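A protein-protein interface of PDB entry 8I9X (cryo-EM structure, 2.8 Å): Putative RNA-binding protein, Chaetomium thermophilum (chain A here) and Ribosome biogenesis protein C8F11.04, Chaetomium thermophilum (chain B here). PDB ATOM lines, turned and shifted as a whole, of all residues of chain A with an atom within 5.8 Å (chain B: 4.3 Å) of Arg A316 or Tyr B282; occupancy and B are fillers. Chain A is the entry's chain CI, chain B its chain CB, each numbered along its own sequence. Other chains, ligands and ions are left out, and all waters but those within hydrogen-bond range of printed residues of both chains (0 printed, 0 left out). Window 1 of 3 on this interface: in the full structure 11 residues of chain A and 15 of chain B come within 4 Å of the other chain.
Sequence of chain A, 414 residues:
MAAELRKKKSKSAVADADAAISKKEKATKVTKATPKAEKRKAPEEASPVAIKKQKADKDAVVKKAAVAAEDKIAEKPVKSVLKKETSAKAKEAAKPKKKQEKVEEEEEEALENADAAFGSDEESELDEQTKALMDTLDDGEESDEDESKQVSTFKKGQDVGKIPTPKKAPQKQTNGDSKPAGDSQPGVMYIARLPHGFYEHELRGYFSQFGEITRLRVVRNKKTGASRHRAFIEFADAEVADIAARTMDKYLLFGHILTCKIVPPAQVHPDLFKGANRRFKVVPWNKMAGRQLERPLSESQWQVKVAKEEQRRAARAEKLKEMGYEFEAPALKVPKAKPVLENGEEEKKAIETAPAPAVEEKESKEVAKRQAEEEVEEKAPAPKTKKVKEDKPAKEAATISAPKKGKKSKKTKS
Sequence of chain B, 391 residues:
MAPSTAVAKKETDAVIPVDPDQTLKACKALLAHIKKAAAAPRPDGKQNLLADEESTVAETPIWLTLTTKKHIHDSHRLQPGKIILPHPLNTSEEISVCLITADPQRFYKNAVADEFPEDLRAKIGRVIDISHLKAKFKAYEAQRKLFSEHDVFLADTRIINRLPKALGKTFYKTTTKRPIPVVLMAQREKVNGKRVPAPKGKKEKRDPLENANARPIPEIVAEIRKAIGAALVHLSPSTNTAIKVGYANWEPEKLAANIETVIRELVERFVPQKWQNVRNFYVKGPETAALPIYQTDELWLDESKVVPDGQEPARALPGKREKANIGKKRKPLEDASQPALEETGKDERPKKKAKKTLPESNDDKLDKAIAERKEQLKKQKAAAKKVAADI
The backbone carbonyl oxygen of Ala B290 sits close to the side-chain amino group of Lys A319 (2.4 Å).
O of Val B283 sits at hydrogen-bond distance from N of Leu B291, 2.8 Å away.
OD1 of Asn B280 sits close to OH of Tyr B282 (3.3 Å).
N of Thr B65 sits at hydrogen-bond distance from O of Tyr B282, 2.8 Å away.
Among the printed residues, merely in contact across the chains: Arg A316 with Tyr B282, Leu A320 with Leu B291, Leu A320 with Ala B290 and Leu A320 with Pro B292.
Arg A316 touches just one residue of chain B: Tyr B282.
Asn B280 touches none of the printed residues of chain A.
Tyr B282 touches just one residue of chain A: Arg A316 (3.6 Å).
Printed residues of chain A within 4 Å of Ala B290: Lys A319 and Leu A320.
Printed residues of chain A within 4 Å of Leu B291: Leu A320.
The nearest printed residue of chain A that does not touch Tyr B282 is Arg A312 (6.3 Å).
The nearest printed residue of chain A that does not touch Ala B290 is Arg A316 (4.2 Å).
Of the 11 printed residues of chain A, 3 touch a printed residue of chain B.
Hydrophobic or aromatic side chains of chain A that line the printed part of chain B: Leu A320.
Of the 10 printed residues of chain B, 4 touch a printed residue of chain A.
Hydrophobic or aromatic side chains of chain B within 4 Å of the printed part of chain A: Tyr B282, Leu B291 and Pro B292.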
ATOM      1  N   GLN A 311      24.918 -12.362   8.025  1.00  0.00           N
ATOM      2  CA  GLN A 311      23.596 -12.896   7.693  1.00  0.00           C
ATOM      3  C   GLN A 311      23.643 -14.422   7.616  1.00  0.00           C
ATOM      4  O   GLN A 311      22.628 -15.098   7.827  1.00  0.00           O
ATOM      5  CB  GLN A 311      23.044 -12.279   6.402  1.00  0.00           C
ATOM      6  CG  GLN A 311      23.780 -12.613   5.129  1.00  0.00           C
ATOM      7  CD  GLN A 311      23.202 -11.922   3.909  1.00  0.00           C
ATOM      8  OE1 GLN A 311      22.202 -11.211   3.996  1.00  0.00           O
ATOM      9  NE2 GLN A 311      23.840 -12.124   2.761  1.00  0.00           N
ATOM     10  N   ARG A 312      24.825 -14.981   7.353  1.00  0.00           N
ATOM     11  CA  ARG A 312      25.034 -16.405   7.594  1.00  0.00           C
ATOM     12  C   ARG A 312      24.823 -16.753   9.065  1.00  0.00           C
ATOM     13  O   ARG A 312      24.222 -17.781   9.384  1.00  0.00           O
ATOM     14  CB  ARG A 312      26.435 -16.821   7.156  1.00  0.00           C
ATOM     15  CG  ARG A 312      26.599 -18.310   6.961  1.00  0.00           C
ATOM     16  CD  ARG A 312      27.654 -18.612   5.918  1.00  0.00           C
ATOM     17  NE  ARG A 312      28.986 -18.194   6.340  1.00  0.00           N
ATOM     18  CZ  ARG A 312      30.109 -18.667   5.820  1.00  0.00           C
ATOM     19  NH1 ARG A 312      30.094 -19.568   4.851  1.00  0.00           N
ATOM     20  NH2 ARG A 312      31.276 -18.227   6.280  1.00  0.00           N
ATOM     21  N   ARG A 313      25.351 -15.930   9.976  1.00  0.00           N
ATOM     22  CA  ARG A 313      25.024 -16.093  11.388  1.00  0.00           C
ATOM     23  C   ARG A 313      23.540 -15.906  11.662  1.00  0.00           C
ATOM     24  O   ARG A 313      23.034 -16.475  12.627  1.00  0.00           O
ATOM     25  CB  ARG A 313      25.799 -15.126  12.298  1.00  0.00           C
ATOM     26  CG  ARG A 313      27.304 -15.325  12.435  1.00  0.00           C
ATOM     27  CD  ARG A 313      27.865 -14.270  13.398  1.00  0.00           C
ATOM     28  NE  ARG A 313      29.298 -14.390  13.632  1.00  0.00           N
ATOM     29  CZ  ARG A 313      30.227 -13.772  12.922  1.00  0.00           C
ATOM     30  NH1 ARG A 313      29.909 -12.938  11.948  1.00  0.00           N
ATOM     31  NH2 ARG A 313      31.508 -13.975  13.215  1.00  0.00           N
ATOM     32  N   ALA A 314      22.844 -15.101  10.865  1.00  0.00           N
ATOM     33  CA  ALA A 314      21.397 -14.982  11.021  1.00  0.00           C
ATOM     34  C   ALA A 314      20.705 -16.289  10.654  1.00  0.00           C
ATOM     35  O   ALA A 314      19.767 -16.724  11.332  1.00  0.00           O
ATOM     36  CB  ALA A 314      20.866 -13.830  10.168  1.00  0.00           C
ATOM     37  N   ALA A 315      21.163 -16.930   9.577  1.00  0.00           N
ATOM     38  CA  ALA A 315      20.674 -18.266   9.239  1.00  0.00           C
ATOM     39  C   ALA A 315      21.021 -19.268  10.336  1.00  0.00           C
ATOM     40  O   ALA A 315      20.208 -20.134  10.692  1.00  0.00           O
ATOM     41  CB  ALA A 315      21.251 -18.713   7.897  1.00  0.00           C
ATOM     42  N   ARG A 316      22.234 -19.166  10.880  1.00  0.00           N
ATOM     43  CA  ARG A 316      22.604 -19.983  12.027  1.00  0.00           C
ATOM     44  C   ARG A 316      21.674 -19.728  13.201  1.00  0.00           C
ATOM     45  O   ARG A 316      21.274 -20.667  13.886  1.00  0.00           O
ATOM     46  CB  ARG A 316      24.052 -19.711  12.437  1.00  0.00           C
ATOM     47  CG  ARG A 316      25.097 -20.158  11.431  1.00  0.00           C
ATOM     48  CD  ARG A 316      26.497 -19.871  11.956  1.00  0.00           C
ATOM     49  NE  ARG A 316      27.540 -20.203  10.993  1.00  0.00           N
ATOM     50  CZ  ARG A 316      28.114 -21.394  10.894  1.00  0.00           C
ATOM     51  NH1 ARG A 316      27.768 -22.394  11.687  1.00  0.00           N
ATOM     52  NH2 ARG A 316      29.059 -21.585   9.979  1.00  0.00           N
ATOM     53  N   ALA A 317      21.312 -18.472  13.441  1.00  0.00           N
ATOM     54  CA  ALA A 317      20.416 -18.147  14.541  1.00  0.00           C
ATOM     55  C   ALA A 317      19.033 -18.736  14.317  1.00  0.00           C
ATOM     56  O   ALA A 317      18.404 -19.227  15.261  1.00  0.00           O
ATOM     57  CB  ALA A 317      20.336 -16.632  14.717  1.00  0.00           C
ATOM     58  N   GLU A 318      18.536 -18.700  13.079  1.00  0.00           N
ATOM     59  CA  GLU A 318      17.195 -19.223  12.843  1.00  0.00           C
ATOM     60  C   GLU A 318      17.179 -20.744  12.939  1.00  0.00           C
ATOM     61  O   GLU A 318      16.169 -21.334  13.339  1.00  0.00           O
ATOM     62  CB  GLU A 318      16.639 -18.748  11.495  1.00  0.00           C
ATOM     63  CG  GLU A 318      17.405 -19.171  10.263  1.00  0.00           C
ATOM     64  CD  GLU A 318      16.998 -20.543   9.753  1.00  0.00           C
ATOM     65  OE1 GLU A 318      15.893 -21.005  10.107  1.00  0.00           O
ATOM     66  OE2 GLU A 318      17.784 -21.155   9.000  1.00  0.00           O
ATOM     67  N   LYS A 319      18.288 -21.402  12.583  1.00  0.00           N
ATOM     68  CA  LYS A 319      18.351 -22.844  12.816  1.00  0.00           C
ATOM     69  C   LYS A 319      18.661 -23.168  14.276  1.00  0.00           C
ATOM     70  O   LYS A 319      18.419 -24.296  14.721  1.00  0.00           O
ATOM     71  CB  LYS A 319      19.366 -23.499  11.873  1.00  0.00           C
ATOM     72  CG  LYS A 319      20.815 -23.092  12.071  1.00  0.00           C
ATOM     73  CD  LYS A 319      21.577 -24.051  12.974  1.00  0.00           C
ATOM     74  CE  LYS A 319      23.039 -23.645  13.076  1.00  0.00           C
ATOM     75  NZ  LYS A 319      23.792 -24.488  14.044  1.00  0.00           N
ATOM     76  N   LEU A 320      19.192 -22.205  15.032  1.00  0.00           N
ATOM     77  CA  LEU A 320      19.453 -22.380  16.457  1.00  0.00           C
ATOM     78  C   LEU A 320      18.271 -21.991  17.335  1.00  0.00           C
ATOM     79  O   LEU A 320      18.317 -22.237  18.546  1.00  0.00           O
ATOM     80  CB  LEU A 320      20.679 -21.562  16.882  1.00  0.00           C
ATOM     81  CG  LEU A 320      22.090 -22.029  16.511  1.00  0.00           C
ATOM     82  CD1 LEU A 320      23.116 -21.006  16.972  1.00  0.00           C
ATOM     83  CD2 LEU A 320      22.404 -23.388  17.101  1.00  0.00           C
ATOM     84  N   LYS A 321      17.232 -21.379  16.774  1.00  0.00           N
ATOM     85  CA  LYS A 321      16.032 -21.109  17.556  1.00  0.00           C
ATOM     86  C   LYS A 321      15.354 -22.400  17.984  1.00  0.00           C
ATOM     87  O   LYS A 321      14.856 -22.498  19.112  1.00  0.00           O
ATOM     88  CB  LYS A 321      15.053 -20.237  16.762  1.00  0.00           C
ATOM     89  CG  LYS A 321      15.547 -18.826  16.452  1.00  0.00           C
ATOM     90  CD  LYS A 321      15.766 -17.992  17.712  1.00  0.00           C
ATOM     91  CE  LYS A 321      17.245 -17.860  18.057  1.00  0.00           C
ATOM     92  NZ  LYS A 321      17.466 -16.957  19.220  1.00  0.00           N
ATOM     93  N   LEU B  64      33.930 -31.516  18.522  1.00  0.00           N
ATOM     94  CA  LEU B  64      34.288 -30.090  18.655  1.00  0.00           C
ATOM     95  C   LEU B  64      35.138 -29.752  17.437  1.00  0.00           C
ATOM     96  O   LEU B  64      36.148 -30.446  17.237  1.00  0.00           O
ATOM     97  CB  LEU B  64      35.138 -29.963  19.915  1.00  0.00           C
ATOM     98  CG  LEU B  64      35.718 -28.579  20.195  1.00  0.00           C
ATOM     99  CD1 LEU B  64      34.622 -27.608  20.605  1.00  0.00           C
ATOM    100  CD2 LEU B  64      36.782 -28.655  21.277  1.00  0.00           C
ATOM    101  N   THR B  65      34.772 -28.741  16.654  1.00  0.00           N
ATOM    102  CA  THR B  65      35.516 -28.464  15.400  1.00  0.00           C
ATOM    103  C   THR B  65      36.262 -27.131  15.469  1.00  0.00           C
ATOM    104  O   THR B  65      35.592 -26.097  15.621  1.00  0.00           O
ATOM    105  CB  THR B  65      34.576 -28.490  14.194  1.00  0.00           C
ATOM    106  OG1 THR B  65      33.436 -27.682  14.492  1.00  0.00           O
ATOM    107  CG2 THR B  65      34.132 -29.889  13.828  1.00  0.00           C
ATOM    108  N   THR B  67      38.138 -24.212  13.581  1.00  0.00           N
ATOM    109  CA  THR B  67      38.254 -23.661  12.221  1.00  0.00           C
ATOM    110  C   THR B  67      39.329 -22.617  12.332  1.00  0.00           C
ATOM    111  O   THR B  67      39.336 -21.891  13.340  1.00  0.00           O
ATOM    112  CB  THR B  67      36.940 -23.008  11.785  1.00  0.00           C
ATOM    113  OG1 THR B  67      35.934 -24.021  11.726  1.00  0.00           O
ATOM    114  CG2 THR B  67      37.048 -22.295  10.456  1.00  0.00           C
ATOM    115  N   ASN B 280      37.111 -19.781  14.574  1.00  0.00           N
ATOM    116  CA  ASN B 280      35.863 -20.328  15.174  1.00  0.00           C
ATOM    117  C   ASN B 280      36.145 -21.644  15.919  1.00  0.00           C
ATOM    118  O   ASN B 280      37.110 -22.330  15.540  1.00  0.00           O
ATOM    119  CB  ASN B 280      34.777 -20.495  14.118  1.00  0.00           C
ATOM    120  CG  ASN B 280      34.123 -19.187  13.729  1.00  0.00           C
ATOM    121  OD1 ASN B 280      33.071 -18.834  14.257  1.00  0.00           O
ATOM    122  ND2 ASN B 280      34.735 -18.462  12.808  1.00  0.00           N
ATOM    123  N   PHE B 281      35.340 -21.987  16.937  1.00  0.00           N
ATOM    124  CA  PHE B 281      35.505 -23.266  17.685  1.00  0.00           C
ATOM    125  C   PHE B 281      34.127 -23.833  18.023  1.00  0.00           C
ATOM    126  O   PHE B 281      33.778 -23.804  19.196  1.00  0.00           O
ATOM    127  CB  PHE B 281      36.361 -23.038  18.926  1.00  0.00           C
ATOM    128  CG  PHE B 281      37.562 -23.934  19.076  1.00  0.00           C
ATOM    129  CD1 PHE B 281      37.420 -25.309  19.150  1.00  0.00           C
ATOM    130  CD2 PHE B 281      38.834 -23.399  19.175  1.00  0.00           C
ATOM    131  CE1 PHE B 281      38.527 -26.130  19.301  1.00  0.00           C
ATOM    132  CE2 PHE B 281      39.939 -24.219  19.330  1.00  0.00           C
ATOM    133  CZ  PHE B 281      39.785 -25.583  19.392  1.00  0.00           C
ATOM    134  N   TYR B 282      33.405 -24.380  17.039  1.00  0.00           N
ATOM    135  CA  TYR B 282      32.011 -24.856  17.239  1.00  0.00           C
ATOM    136  C   TYR B 282      31.917 -26.268  17.817  1.00  0.00           C
ATOM    137  O   TYR B 282      32.917 -26.988  17.764  1.00  0.00           O
ATOM    138  CB  TYR B 282      31.247 -24.954  15.918  1.00  0.00           C
ATOM    139  CG  TYR B 282      31.468 -23.880  14.883  1.00  0.00           C
ATOM    140  CD1 TYR B 282      30.673 -22.748  14.852  1.00  0.00           C
ATOM    141  CD2 TYR B 282      32.415 -24.032  13.887  1.00  0.00           C
ATOM    142  CE1 TYR B 282      30.846 -21.770  13.886  1.00  0.00           C
ATOM    143  CE2 TYR B 282      32.603 -23.066  12.914  1.00  0.00           C
ATOM    144  CZ  TYR B 282      31.813 -21.931  12.911  1.00  0.00           C
ATOM    145  OH  TYR B 282      31.992 -20.972  11.958  1.00  0.00           O
ATOM    146  N   VAL B 283      30.738 -26.647  18.336  1.00  0.00           N
ATOM    147  CA  VAL B 283      30.486 -28.031  18.843  1.00  0.00           C
ATOM    148  C   VAL B 283      29.584 -28.708  17.813  1.00  0.00           C
ATOM    149  O   VAL B 283      28.753 -27.996  17.222  1.00  0.00           O
ATOM    150  CB  VAL B 283      29.873 -28.052  20.255  1.00  0.00           C
ATOM    151  CG1 VAL B 283      29.755 -29.454  20.823  1.00  0.00           C
ATOM    152  CG2 VAL B 283      30.643 -27.159  21.213  1.00  0.00           C
ATOM    153  N   ALA B 290      25.737 -27.074  13.967  1.00  0.00           N
ATOM    154  CA  ALA B 290      26.897 -26.613  14.713  1.00  0.00           C
ATOM    155  C   ALA B 290      26.485 -25.606  15.777  1.00  0.00           C
ATOM    156  O   ALA B 290      25.544 -24.827  15.591  1.00  0.00           O
ATOM    157  CB  ALA B 290      27.934 -25.975  13.782  1.00  0.00           C
ATOM    158  N   LEU B 291      27.200 -25.632  16.899  1.00  0.00           N
ATOM    159  CA  LEU B 291      27.014 -24.669  17.983  1.00  0.00           C
ATOM    160  C   LEU B 291      28.214 -23.736  18.005  1.00  0.00           C
ATOM    161  O   LEU B 291      29.331 -24.171  18.337  1.00  0.00           O
ATOM    162  CB  LEU B 291      26.870 -25.385  19.323  1.00  0.00           C
ATOM    163  CG  LEU B 291      25.627 -26.254  19.488  1.00  0.00           C
ATOM    164  CD1 LEU B 291      25.700 -26.997  20.800  1.00  0.00           C
ATOM    165  CD2 LEU B 291      24.362 -25.417  19.406  1.00  0.00           C
ATOM    166  N   PRO B 292      28.099 -22.411  17.787  1.00  0.00           N
ATOM    167  CA  PRO B 292      29.271 -21.555  17.931  1.00  0.00           C
ATOM    168  C   PRO B 292      29.882 -21.434  19.337  1.00  0.00           C
ATOM    169  O   PRO B 292      29.173 -21.665  20.274  1.00  0.00           O
ATOM    170  CB  PRO B 292      28.749 -20.174  17.499  1.00  0.00           C
ATOM    171  CG  PRO B 292      27.567 -20.477  16.622  1.00  0.00           C
ATOM    172  CD  PRO B 292      26.922 -21.649  17.322  1.00  0.00           C
